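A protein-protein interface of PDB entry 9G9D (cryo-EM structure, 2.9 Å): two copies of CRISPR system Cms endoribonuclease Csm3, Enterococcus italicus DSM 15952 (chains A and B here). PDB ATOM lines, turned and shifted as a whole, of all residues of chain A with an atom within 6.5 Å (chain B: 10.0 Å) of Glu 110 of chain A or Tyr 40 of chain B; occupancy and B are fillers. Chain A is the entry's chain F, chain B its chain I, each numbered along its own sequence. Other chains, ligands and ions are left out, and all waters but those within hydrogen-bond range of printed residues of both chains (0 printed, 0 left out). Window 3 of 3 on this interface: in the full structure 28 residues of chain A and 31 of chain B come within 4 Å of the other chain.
The side-chain hydroxyl (OH) of Tyr 40 of chain B is in hydrogen-bond range of the side-chain carboxylate (OE2) of Glu 110 of chain A (2.5 Å). The side-chain amino group (NZ) of Lys 114 of chain A sits at hydrogen-bond distance from the backbone carbonyl oxygen (O) of Tyr 40 of chain B (2.5 Å). OD2 of Asp 38 of chain B is in salt-bridge range of NH1 of Arg 144 of chain A, 2.6 Å away.
The backbone carbonyl oxygen (O) of Phe 111 of chain A is in hydrogen-bond range of the backbone NH (N) of Leu 116 of chain A (3.0 Å). OD2 of Asp 38 of chain B sits at hydrogen-bond distance from OG of Ser 41 of chain B (3.1 Å). The backbone carbonyl oxygen of Leu 43 of chain B lies within hydrogen-bond range of the backbone NH of Asp 38 of chain B (2.8 Å).
Leu 116 of chain A touches Pro 39 of chain B. Leu 116 of chain A touches Tyr 40 of chain B (CD2 to CA, 3.6 Å). Thr 143 of chain A touches Pro 39 of chain B. Thr 143 of chain A touches Tyr 40 of chain B. Arg 144 of chain A touches Tyr 40 of chain B. Arg 144 of chain A touches Ser 41 of chain B. Arg 144 of chain A touches Phe 102 of chain B.
Of chain B, only Tyr 40 comes within 4 Å of Glu 110 of chain A. Of the printed residues of chain A, Tyr 40 of chain B touches Glu 110 (2.5 Å), Lys 114 (2.5 Å), Leu 116 (3.6 Å), Thr 143 (3.99 Å) and Arg 144 (3.4 Å). No residue of chain B comes within 4 Å of Ser 107 of chain A. No residue of chain B comes within 4 Å of Lys 113 of chain A. No residue of chain B comes within 4 Å of Gly 145 of chain A. Of the printed residues of chain B, Leu 116 of chain A touches Pro 39 (3.3 Å) and Tyr 40 (3.6 Å). Of the printed residues of chain A, Phe 102 of chain B touches Arg 144 (3.5 Å). Arg 37 of chain B touches none of the printed residues of chain A. Lys 105 of chain B touches none of the printed residues of chain A.
Of the 13 printed residues of chain B, 5 touch a printed residue of chain A. Printed residues of chain B that touch a printed residue of chain A: Asp 38, Pro 39, Tyr 40, Ser 41 and Phe 102. Hydrophobic or aromatic side chains of chain B that line the printed part of chain A: Pro 39, Tyr 40 and Phe 102. Hydrophobic or aromatic side chains of chain A within 4 Å of the printed part of chain B: Leu 116. Among the printed residues, Asp or Glu carboxylates within 4 Å of a Lys or Arg side-chain nitrogen of the other chain: Arg 144 of chain A with Asp 38 of chain B.
2 positions are printed for both chains.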
ATOM      1  N   LYS A 105     -28.560  -9.673 -13.642  1.00  0.00           N
ATOM      2  CA  LYS A 105     -29.547 -10.662 -13.227  1.00  0.00           C
ATOM      3  C   LYS A 105     -29.712 -11.757 -14.270  1.00  0.00           C
ATOM      4  O   LYS A 105     -29.951 -12.918 -13.915  1.00  0.00           O
ATOM      5  CB  LYS A 105     -30.882  -9.978 -12.949  1.00  0.00           C
ATOM      6  CG  LYS A 105     -31.838 -10.810 -12.121  1.00  0.00           C
ATOM      7  CD  LYS A 105     -32.937  -9.945 -11.533  1.00  0.00           C
ATOM      8  CE  LYS A 105     -32.355  -8.779 -10.751  1.00  0.00           C
ATOM      9  NZ  LYS A 105     -31.440  -9.225  -9.666  1.00  0.00           N
ATOM     10  N   ALA A 106     -29.585 -11.413 -15.552  1.00  0.00           N
ATOM     11  CA  ALA A 106     -29.630 -12.426 -16.598  1.00  0.00           C
ATOM     12  C   ALA A 106     -28.469 -13.401 -16.461  1.00  0.00           C
ATOM     13  O   ALA A 106     -28.646 -14.615 -16.597  1.00  0.00           O
ATOM     14  CB  ALA A 106     -29.621 -11.764 -17.975  1.00  0.00           C
ATOM     15  N   SER A 107     -27.272 -12.887 -16.174  1.00  0.00           N
ATOM     16  CA  SER A 107     -26.123 -13.761 -15.964  1.00  0.00           C
ATOM     17  C   SER A 107     -26.291 -14.605 -14.707  1.00  0.00           C
ATOM     18  O   SER A 107     -25.883 -15.771 -14.676  1.00  0.00           O
ATOM     19  CB  SER A 107     -24.843 -12.931 -15.887  1.00  0.00           C
ATOM     20  OG  SER A 107     -23.740 -13.740 -15.532  1.00  0.00           O
ATOM     21  N   GLN A 108     -26.888 -14.034 -13.660  1.00  0.00           N
ATOM     22  CA  GLN A 108     -27.139 -14.797 -12.442  1.00  0.00           C
ATOM     23  C   GLN A 108     -28.093 -15.955 -12.710  1.00  0.00           C
ATOM     24  O   GLN A 108     -27.861 -17.085 -12.261  1.00  0.00           O
ATOM     25  CB  GLN A 108     -27.694 -13.875 -11.356  1.00  0.00           C
ATOM     26  CG  GLN A 108     -27.932 -14.556 -10.023  1.00  0.00           C
ATOM     27  CD  GLN A 108     -28.356 -13.585  -8.942  1.00  0.00           C
ATOM     28  OE1 GLN A 108     -28.515 -12.391  -9.193  1.00  0.00           O
ATOM     29  NE2 GLN A 108     -28.540 -14.093  -7.729  1.00  0.00           N
ATOM     30  N   GLU A 109     -29.170 -15.694 -13.454  1.00  0.00           N
ATOM     31  CA  GLU A 109     -30.110 -16.761 -13.783  1.00  0.00           C
ATOM     32  C   GLU A 109     -29.476 -17.788 -14.714  1.00  0.00           C
ATOM     33  O   GLU A 109     -29.746 -18.989 -14.602  1.00  0.00           O
ATOM     34  CB  GLU A 109     -31.378 -16.172 -14.398  1.00  0.00           C
ATOM     35  CG  GLU A 109     -32.196 -15.332 -13.425  1.00  0.00           C
ATOM     36  CD  GLU A 109     -33.516 -14.871 -14.009  1.00  0.00           C
ATOM     37  OE1 GLU A 109     -33.770 -15.156 -15.198  1.00  0.00           O
ATOM     38  OE2 GLU A 109     -34.299 -14.226 -13.281  1.00  0.00           O
ATOM     39  N   GLU A 110     -28.627 -17.335 -15.639  1.00  0.00           N
ATOM     40  CA  GLU A 110     -27.928 -18.258 -16.527  1.00  0.00           C
ATOM     41  C   GLU A 110     -27.001 -19.184 -15.748  1.00  0.00           C
ATOM     42  O   GLU A 110     -26.927 -20.385 -16.031  1.00  0.00           O
ATOM     43  CB  GLU A 110     -27.150 -17.468 -17.576  1.00  0.00           C
ATOM     44  CG  GLU A 110     -26.038 -18.229 -18.265  1.00  0.00           C
ATOM     45  CD  GLU A 110     -25.247 -17.344 -19.207  1.00  0.00           C
ATOM     46  OE1 GLU A 110     -25.863 -16.493 -19.880  1.00  0.00           O
ATOM     47  OE2 GLU A 110     -24.009 -17.487 -19.266  1.00  0.00           O
ATOM     48  N   PHE A 111     -26.277 -18.640 -14.769  1.00  0.00           N
ATOM     49  CA  PHE A 111     -25.404 -19.471 -13.945  1.00  0.00           C
ATOM     50  C   PHE A 111     -26.207 -20.417 -13.062  1.00  0.00           C
ATOM     51  O   PHE A 111     -25.808 -21.569 -12.859  1.00  0.00           O
ATOM     52  CB  PHE A 111     -24.484 -18.590 -13.103  1.00  0.00           C
ATOM     53  CG  PHE A 111     -23.228 -18.184 -13.810  1.00  0.00           C
ATOM     54  CD1 PHE A 111     -23.283 -17.509 -15.012  1.00  0.00           C
ATOM     55  CD2 PHE A 111     -21.993 -18.475 -13.270  1.00  0.00           C
ATOM     56  CE1 PHE A 111     -22.131 -17.137 -15.660  1.00  0.00           C
ATOM     57  CE2 PHE A 111     -20.841 -18.104 -13.916  1.00  0.00           C
ATOM     58  CZ  PHE A 111     -20.908 -17.434 -15.110  1.00  0.00           C
ATOM     59  N   ASP A 112     -27.339 -19.953 -12.525  1.00  0.00           N
ATOM     60  CA  ASP A 112     -28.202 -20.844 -11.755  1.00  0.00           C
ATOM     61  C   ASP A 112     -28.789 -21.946 -12.628  1.00  0.00           C
ATOM     62  O   ASP A 112     -29.125 -23.024 -12.126  1.00  0.00           O
ATOM     63  CB  ASP A 112     -29.322 -20.047 -11.086  1.00  0.00           C
ATOM     64  CG  ASP A 112     -28.816 -19.162  -9.966  1.00  0.00           C
ATOM     65  OD1 ASP A 112     -27.601 -19.196  -9.683  1.00  0.00           O
ATOM     66  OD2 ASP A 112     -29.634 -18.434  -9.365  1.00  0.00           O
ATOM     67  N   LYS A 113     -28.934 -21.688 -13.929  1.00  0.00           N
ATOM     68  CA  LYS A 113     -29.395 -22.720 -14.850  1.00  0.00           C
ATOM     69  C   LYS A 113     -28.413 -23.883 -14.907  1.00  0.00           C
ATOM     70  O   LYS A 113     -28.817 -25.051 -14.900  1.00  0.00           O
ATOM     71  CB  LYS A 113     -29.591 -22.116 -16.241  1.00  0.00           C
ATOM     72  CG  LYS A 113     -30.978 -22.281 -16.829  1.00  0.00           C
ATOM     73  CD  LYS A 113     -31.201 -21.274 -17.951  1.00  0.00           C
ATOM     74  CE  LYS A 113     -30.039 -21.280 -18.937  1.00  0.00           C
ATOM     75  NZ  LYS A 113     -30.131 -20.183 -19.944  1.00  0.00           N
ATOM     76  N   LYS A 114     -27.118 -23.579 -14.956  1.00  0.00           N
ATOM     77  CA  LYS A 114     -26.072 -24.589 -15.056  1.00  0.00           C
ATOM     78  C   LYS A 114     -25.622 -25.119 -13.702  1.00  0.00           C
ATOM     79  O   LYS A 114     -24.761 -26.005 -13.665  1.00  0.00           O
ATOM     80  CB  LYS A 114     -24.867 -24.014 -15.802  1.00  0.00           C
ATOM     81  CG  LYS A 114     -25.226 -23.311 -17.098  1.00  0.00           C
ATOM     82  CD  LYS A 114     -24.040 -22.561 -17.685  1.00  0.00           C
ATOM     83  CE  LYS A 114     -23.129 -23.471 -18.493  1.00  0.00           C
ATOM     84  NZ  LYS A 114     -22.294 -24.365 -17.647  1.00  0.00           N
ATOM     85  N   ASP A 115     -26.180 -24.607 -12.603  1.00  0.00           N
ATOM     86  CA  ASP A 115     -25.707 -24.920 -11.255  1.00  0.00           C
ATOM     87  C   ASP A 115     -24.213 -24.620 -11.133  1.00  0.00           C
ATOM     88  O   ASP A 115     -23.409 -25.467 -10.743  1.00  0.00           O
ATOM     89  CB  ASP A 115     -26.015 -26.372 -10.878  1.00  0.00           C
ATOM     90  CG  ASP A 115     -25.808 -26.647  -9.401  1.00  0.00           C
ATOM     91  OD1 ASP A 115     -26.632 -26.180  -8.587  1.00  0.00           O
ATOM     92  OD2 ASP A 115     -24.820 -27.327  -9.054  1.00  0.00           O
ATOM     93  N   LEU A 116     -23.850 -23.389 -11.481  1.00  0.00           N
ATOM     94  CA  LEU A 116     -22.465 -22.953 -11.537  1.00  0.00           C
ATOM     95  C   LEU A 116     -22.255 -21.778 -10.593  1.00  0.00           C
ATOM     96  O   LEU A 116     -23.118 -20.905 -10.460  1.00  0.00           O
ATOM     97  CB  LEU A 116     -22.076 -22.555 -12.965  1.00  0.00           C
ATOM     98  CG  LEU A 116     -20.622 -22.165 -13.222  1.00  0.00           C
ATOM     99  CD1 LEU A 116     -19.706 -23.348 -12.987  1.00  0.00           C
ATOM    100  CD2 LEU A 116     -20.466 -21.647 -14.633  1.00  0.00           C
ATOM    101  N   THR A 143     -16.305 -16.046 -12.790  1.00  0.00           N
ATOM    102  CA  THR A 143     -16.294 -17.051 -13.882  1.00  0.00           C
ATOM    103  C   THR A 143     -16.498 -16.391 -15.231  1.00  0.00           C
ATOM    104  O   THR A 143     -17.303 -15.443 -15.309  1.00  0.00           O
ATOM    105  CB  THR A 143     -17.356 -18.115 -13.604  1.00  0.00           C
ATOM    106  OG1 THR A 143     -17.053 -18.624 -12.308  1.00  0.00           O
ATOM    107  CG2 THR A 143     -17.335 -19.250 -14.613  1.00  0.00           C
ATOM    108  N   ARG A 144     -15.791 -16.865 -16.262  1.00  0.00           N
ATOM    109  CA  ARG A 144     -15.998 -16.349 -17.637  1.00  0.00           C
ATOM    110  C   ARG A 144     -17.451 -16.619 -18.045  1.00  0.00           C
ATOM    111  O   ARG A 144     -18.002 -17.658 -17.628  1.00  0.00           O
ATOM    112  CB  ARG A 144     -15.076 -17.058 -18.631  1.00  0.00           C
ATOM    113  CG  ARG A 144     -15.402 -16.786 -20.091  1.00  0.00           C
ATOM    114  CD  ARG A 144     -15.036 -17.929 -21.014  1.00  0.00           C
ATOM    115  NE  ARG A 144     -15.767 -19.164 -20.715  1.00  0.00           N
ATOM    116  CZ  ARG A 144     -16.587 -19.754 -21.571  1.00  0.00           C
ATOM    117  NH1 ARG A 144     -16.733 -21.067 -21.555  1.00  0.00           N
ATOM    118  NH2 ARG A 144     -17.248 -19.030 -22.455  1.00  0.00           N
ATOM    119  N   GLY A 145     -18.040 -15.729 -18.839  1.00  0.00           N
ATOM    120  CA  GLY A 145     -19.429 -15.919 -19.287  1.00  0.00           C
ATOM    121  C   GLY A 145     -20.356 -15.136 -18.391  1.00  0.00           C
ATOM    122  O   GLY A 145     -21.585 -15.270 -18.541  1.00  0.00           O
ATOM    123  N   ALA A 146     -19.780 -14.342 -17.487  1.00  0.00           N
ATOM    124  CA  ALA A 146     -20.605 -13.503 -16.588  1.00  0.00           C
ATOM    125  C   ALA A 146     -20.674 -12.084 -17.154  1.00  0.00           C
ATOM    126  O   ALA A 146     -19.709 -11.651 -17.814  1.00  0.00           O
ATOM    127  CB  ALA A 146     -20.037 -13.514 -15.192  1.00  0.00           C
ATOM    128  N   VAL B  36      -7.072 -28.522 -14.886  1.00  0.00           N
ATOM    129  CA  VAL B  36      -7.771 -27.254 -14.730  1.00  0.00           C
ATOM    130  C   VAL B  36      -8.769 -27.090 -15.868  1.00  0.00           C
ATOM    131  O   VAL B  36      -8.457 -27.330 -17.042  1.00  0.00           O
ATOM    132  CB  VAL B  36      -6.774 -26.084 -14.664  1.00  0.00           C
ATOM    133  CG1 VAL B  36      -5.967 -25.977 -15.946  1.00  0.00           C
ATOM    134  CG2 VAL B  36      -7.499 -24.783 -14.384  1.00  0.00           C
ATOM    135  N   ARG B  37      -9.993 -26.711 -15.518  1.00  0.00           N
ATOM    136  CA  ARG B  37     -11.073 -26.618 -16.486  1.00  0.00           C
ATOM    137  C   ARG B  37     -11.786 -25.286 -16.327  1.00  0.00           C
ATOM    138  O   ARG B  37     -11.864 -24.734 -15.227  1.00  0.00           O
ATOM    139  CB  ARG B  37     -12.078 -27.764 -16.325  1.00  0.00           C
ATOM    140  CG  ARG B  37     -11.493 -29.136 -16.575  1.00  0.00           C
ATOM    141  CD  ARG B  37     -12.588 -30.163 -16.758  1.00  0.00           C
ATOM    142  NE  ARG B  37     -12.048 -31.486 -17.042  1.00  0.00           N
ATOM    143  CZ  ARG B  37     -12.758 -32.491 -17.530  1.00  0.00           C
ATOM    144  NH1 ARG B  37     -14.042 -32.354 -17.821  1.00  0.00           N
ATOM    145  NH2 ARG B  37     -12.167 -33.664 -17.736  1.00  0.00           N
ATOM    146  N   ASP B  38     -12.296 -24.776 -17.436  1.00  0.00           N
ATOM    147  CA  ASP B  38     -13.109 -23.573 -17.399  1.00  0.00           C
ATOM    148  C   ASP B  38     -14.461 -23.907 -16.787  1.00  0.00           C
ATOM    149  O   ASP B  38     -15.168 -24.772 -17.318  1.00  0.00           O
ATOM    150  CB  ASP B  38     -13.283 -23.007 -18.800  1.00  0.00           C
ATOM    151  CG  ASP B  38     -14.338 -21.933 -18.860  1.00  0.00           C
ATOM    152  OD1 ASP B  38     -14.206 -20.933 -18.125  1.00  0.00           O
ATOM    153  OD2 ASP B  38     -15.301 -22.087 -19.640  1.00  0.00           O
ATOM    154  N   PRO B  39     -14.859 -23.265 -15.687  1.00  0.00           N
ATOM    155  CA  PRO B  39     -16.102 -23.673 -15.013  1.00  0.00           C
ATOM    156  C   PRO B  39     -17.336 -23.582 -15.889  1.00  0.00           C
ATOM    157  O   PRO B  39     -18.245 -24.411 -15.757  1.00  0.00           O
ATOM    158  CB  PRO B  39     -16.180 -22.706 -13.824  1.00  0.00           C
ATOM    159  CG  PRO B  39     -14.786 -22.271 -13.597  1.00  0.00           C
ATOM    160  CD  PRO B  39     -14.156 -22.204 -14.950  1.00  0.00           C
ATOM    161  N   TYR B  40     -17.394 -22.601 -16.787  1.00  0.00           N
ATOM    162  CA  TYR B  40     -18.588 -22.374 -17.590  1.00  0.00           C
ATOM    163  C   TYR B  40     -18.898 -23.566 -18.486  1.00  0.00           C
ATOM    164  O   TYR B  40     -19.947 -24.201 -18.342  1.00  0.00           O
ATOM    165  CB  TYR B  40     -18.431 -21.105 -18.428  1.00  0.00           C
ATOM    166  CG  TYR B  40     -19.725 -20.635 -19.039  1.00  0.00           C
ATOM    167  CD1 TYR B  40     -20.770 -20.200 -18.238  1.00  0.00           C
ATOM    168  CD2 TYR B  40     -19.904 -20.624 -20.414  1.00  0.00           C
ATOM    169  CE1 TYR B  40     -21.957 -19.772 -18.787  1.00  0.00           C
ATOM    170  CE2 TYR B  40     -21.088 -20.196 -20.974  1.00  0.00           C
ATOM    171  CZ  TYR B  40     -22.112 -19.771 -20.155  1.00  0.00           C
ATOM    172  OH  TYR B  40     -23.296 -19.342 -20.708  1.00  0.00           O
ATOM    173  N   SER B  41     -17.994 -23.882 -19.406  1.00  0.00           N
ATOM    174  CA  SER B  41     -18.194 -24.982 -20.338  1.00  0.00           C
ATOM    175  C   SER B  41     -17.771 -26.332 -19.774  1.00  0.00           C
ATOM    176  O   SER B  41     -18.066 -27.358 -20.393  1.00  0.00           O
ATOM    177  CB  SER B  41     -17.435 -24.711 -21.640  1.00  0.00           C
ATOM    178  OG  SER B  41     -16.045 -24.581 -21.405  1.00  0.00           O
ATOM    179  N   ARG B  42     -17.117 -26.357 -18.610  1.00  0.00           N
ATOM    180  CA  ARG B  42     -16.555 -27.584 -18.040  1.00  0.00           C
ATOM    181  C   ARG B  42     -15.623 -28.272 -19.033  1.00  0.00           C
ATOM    182  O   ARG B  42     -15.623 -29.496 -19.173  1.00  0.00           O
ATOM    183  CB  ARG B  42     -17.653 -28.541 -17.566  1.00  0.00           C
ATOM    184  CG  ARG B  42     -18.519 -27.986 -16.449  1.00  0.00           C
ATOM    185  CD  ARG B  42     -19.179 -29.096 -15.641  1.00  0.00           C
ATOM    186  NE  ARG B  42     -18.201 -29.887 -14.902  1.00  0.00           N
ATOM    187  CZ  ARG B  42     -17.780 -31.092 -15.265  1.00  0.00           C
ATOM    188  NH1 ARG B  42     -18.255 -31.696 -16.341  1.00  0.00           N
ATOM    189  NH2 ARG B  42     -16.859 -31.706 -14.527  1.00  0.00           N
ATOM    190  N   LEU B  43     -14.822 -27.471 -19.728  1.00  0.00           N
ATOM    191  CA  LEU B  43     -13.868 -27.929 -20.720  1.00  0.00           C
ATOM    192  C   LEU B  43     -12.448 -27.640 -20.251  1.00  0.00           C
ATOM    193  O   LEU B  43     -12.221 -26.675 -19.516  1.00  0.00           O
ATOM    194  CB  LEU B  43     -14.105 -27.240 -22.070  1.00  0.00           C
ATOM    195  CG  LEU B  43     -14.913 -27.969 -23.146  1.00  0.00           C
ATOM    196  CD1 LEU B  43     -16.194 -28.544 -22.587  1.00  0.00           C
ATOM    197  CD2 LEU B  43     -15.221 -27.026 -24.291  1.00  0.00           C
ATOM    198  N   PRO B  44     -11.474 -28.452 -20.658  1.00  0.00           N
ATOM    199  CA  PRO B  44     -10.086 -28.182 -20.269  1.00  0.00           C
ATOM    200  C   PRO B  44      -9.612 -26.836 -20.798  1.00  0.00           C
ATOM    201  O   PRO B  44     -10.084 -26.344 -21.825  1.00  0.00           O
ATOM    202  CB  PRO B  44      -9.305 -29.345 -20.896  1.00  0.00           C
ATOM    203  CG  PRO B  44     -10.198 -29.878 -21.961  1.00  0.00           C
ATOM    204  CD  PRO B  44     -11.590 -29.680 -21.459  1.00  0.00           C
ATOM    205  N   ILE B  45      -8.692 -26.210 -20.066  1.00  0.00           N
ATOM    206  CA  ILE B  45      -8.223 -24.849 -20.454  1.00  0.00           C
ATOM    207  C   ILE B  45      -6.724 -24.757 -20.157  1.00  0.00           C
ATOM    208  O   ILE B  45      -6.252 -25.497 -19.266  1.00  0.00           O
ATOM    209  CB  ILE B  45      -9.009 -23.781 -19.673  1.00  0.00           C
ATOM    210  CG1 ILE B  45      -8.664 -22.363 -20.116  1.00  0.00           C
ATOM    211  CG2 ILE B  45      -8.827 -23.952 -18.164  1.00  0.00           C
ATOM    212  CD1 ILE B  45      -9.213 -21.293 -19.193  1.00  0.00           C
ATOM    213  N   PHE B 102      -8.632 -21.066 -24.313  1.00  0.00           N
ATOM    214  CA  PHE B 102      -9.814 -21.888 -24.124  1.00  0.00           C
ATOM    215  C   PHE B 102      -9.849 -23.024 -25.140  1.00  0.00           C
ATOM    216  O   PHE B 102      -9.092 -23.049 -26.113  1.00  0.00           O
ATOM    217  CB  PHE B 102     -11.079 -21.042 -24.236  1.00  0.00           C
ATOM    218  CG  PHE B 102     -11.222 -20.026 -23.145  1.00  0.00           C
ATOM    219  CD1 PHE B 102     -11.778 -20.373 -21.928  1.00  0.00           C
ATOM    220  CD2 PHE B 102     -10.808 -18.721 -23.339  1.00  0.00           C
ATOM    221  CE1 PHE B 102     -11.915 -19.441 -20.925  1.00  0.00           C
ATOM    222  CE2 PHE B 102     -10.942 -17.786 -22.339  1.00  0.00           C
ATOM    223  CZ  PHE B 102     -11.496 -18.146 -21.131  1.00  0.00           C
ATOM    224  N   LYS B 105     -13.561 -24.502 -30.554  1.00  0.00           N
ATOM    225  CA  LYS B 105     -14.831 -25.095 -30.961  1.00  0.00           C
ATOM    226  C   LYS B 105     -14.633 -26.109 -32.079  1.00  0.00           C
ATOM    227  O   LYS B 105     -15.333 -27.127 -32.131  1.00  0.00           O
ATOM    228  CB  LYS B 105     -15.810 -24.003 -31.388  1.00  0.00           C
ATOM    229  CG  LYS B 105     -16.822 -23.630 -30.318  1.00  0.00           C
ATOM    230  CD  LYS B 105     -16.143 -23.277 -29.005  1.00  0.00           C
ATOM    231  CE  LYS B 105     -17.161 -23.071 -27.896  1.00  0.00           C
ATOM    232  NZ  LYS B 105     -16.502 -22.834 -26.585  1.00  0.00           N
ATOM    233  N   GLN B 108     -13.461 -29.183 -30.453  1.00  0.00           N
ATOM    234  CA  GLN B 108     -14.546 -29.749 -29.659  1.00  0.00           C
ATOM    235  C   GLN B 108     -15.526 -30.521 -30.534  1.00  0.00           C
ATOM    236  O   GLN B 108     -15.933 -31.638 -30.190  1.00  0.00           O
ATOM    237  CB  GLN B 108     -15.265 -28.642 -28.893  1.00  0.00           C
ATOM    238  CG  GLN B 108     -16.397 -29.137 -28.023  1.00  0.00           C
ATOM    239  CD  GLN B 108     -17.051 -28.023 -27.244  1.00  0.00           C
ATOM    240  OE1 GLN B 108     -16.658 -26.861 -27.352  1.00  0.00           O
ATOM    241  NE2 GLN B 108     -18.056 -28.367 -26.450  1.00  0.00           N
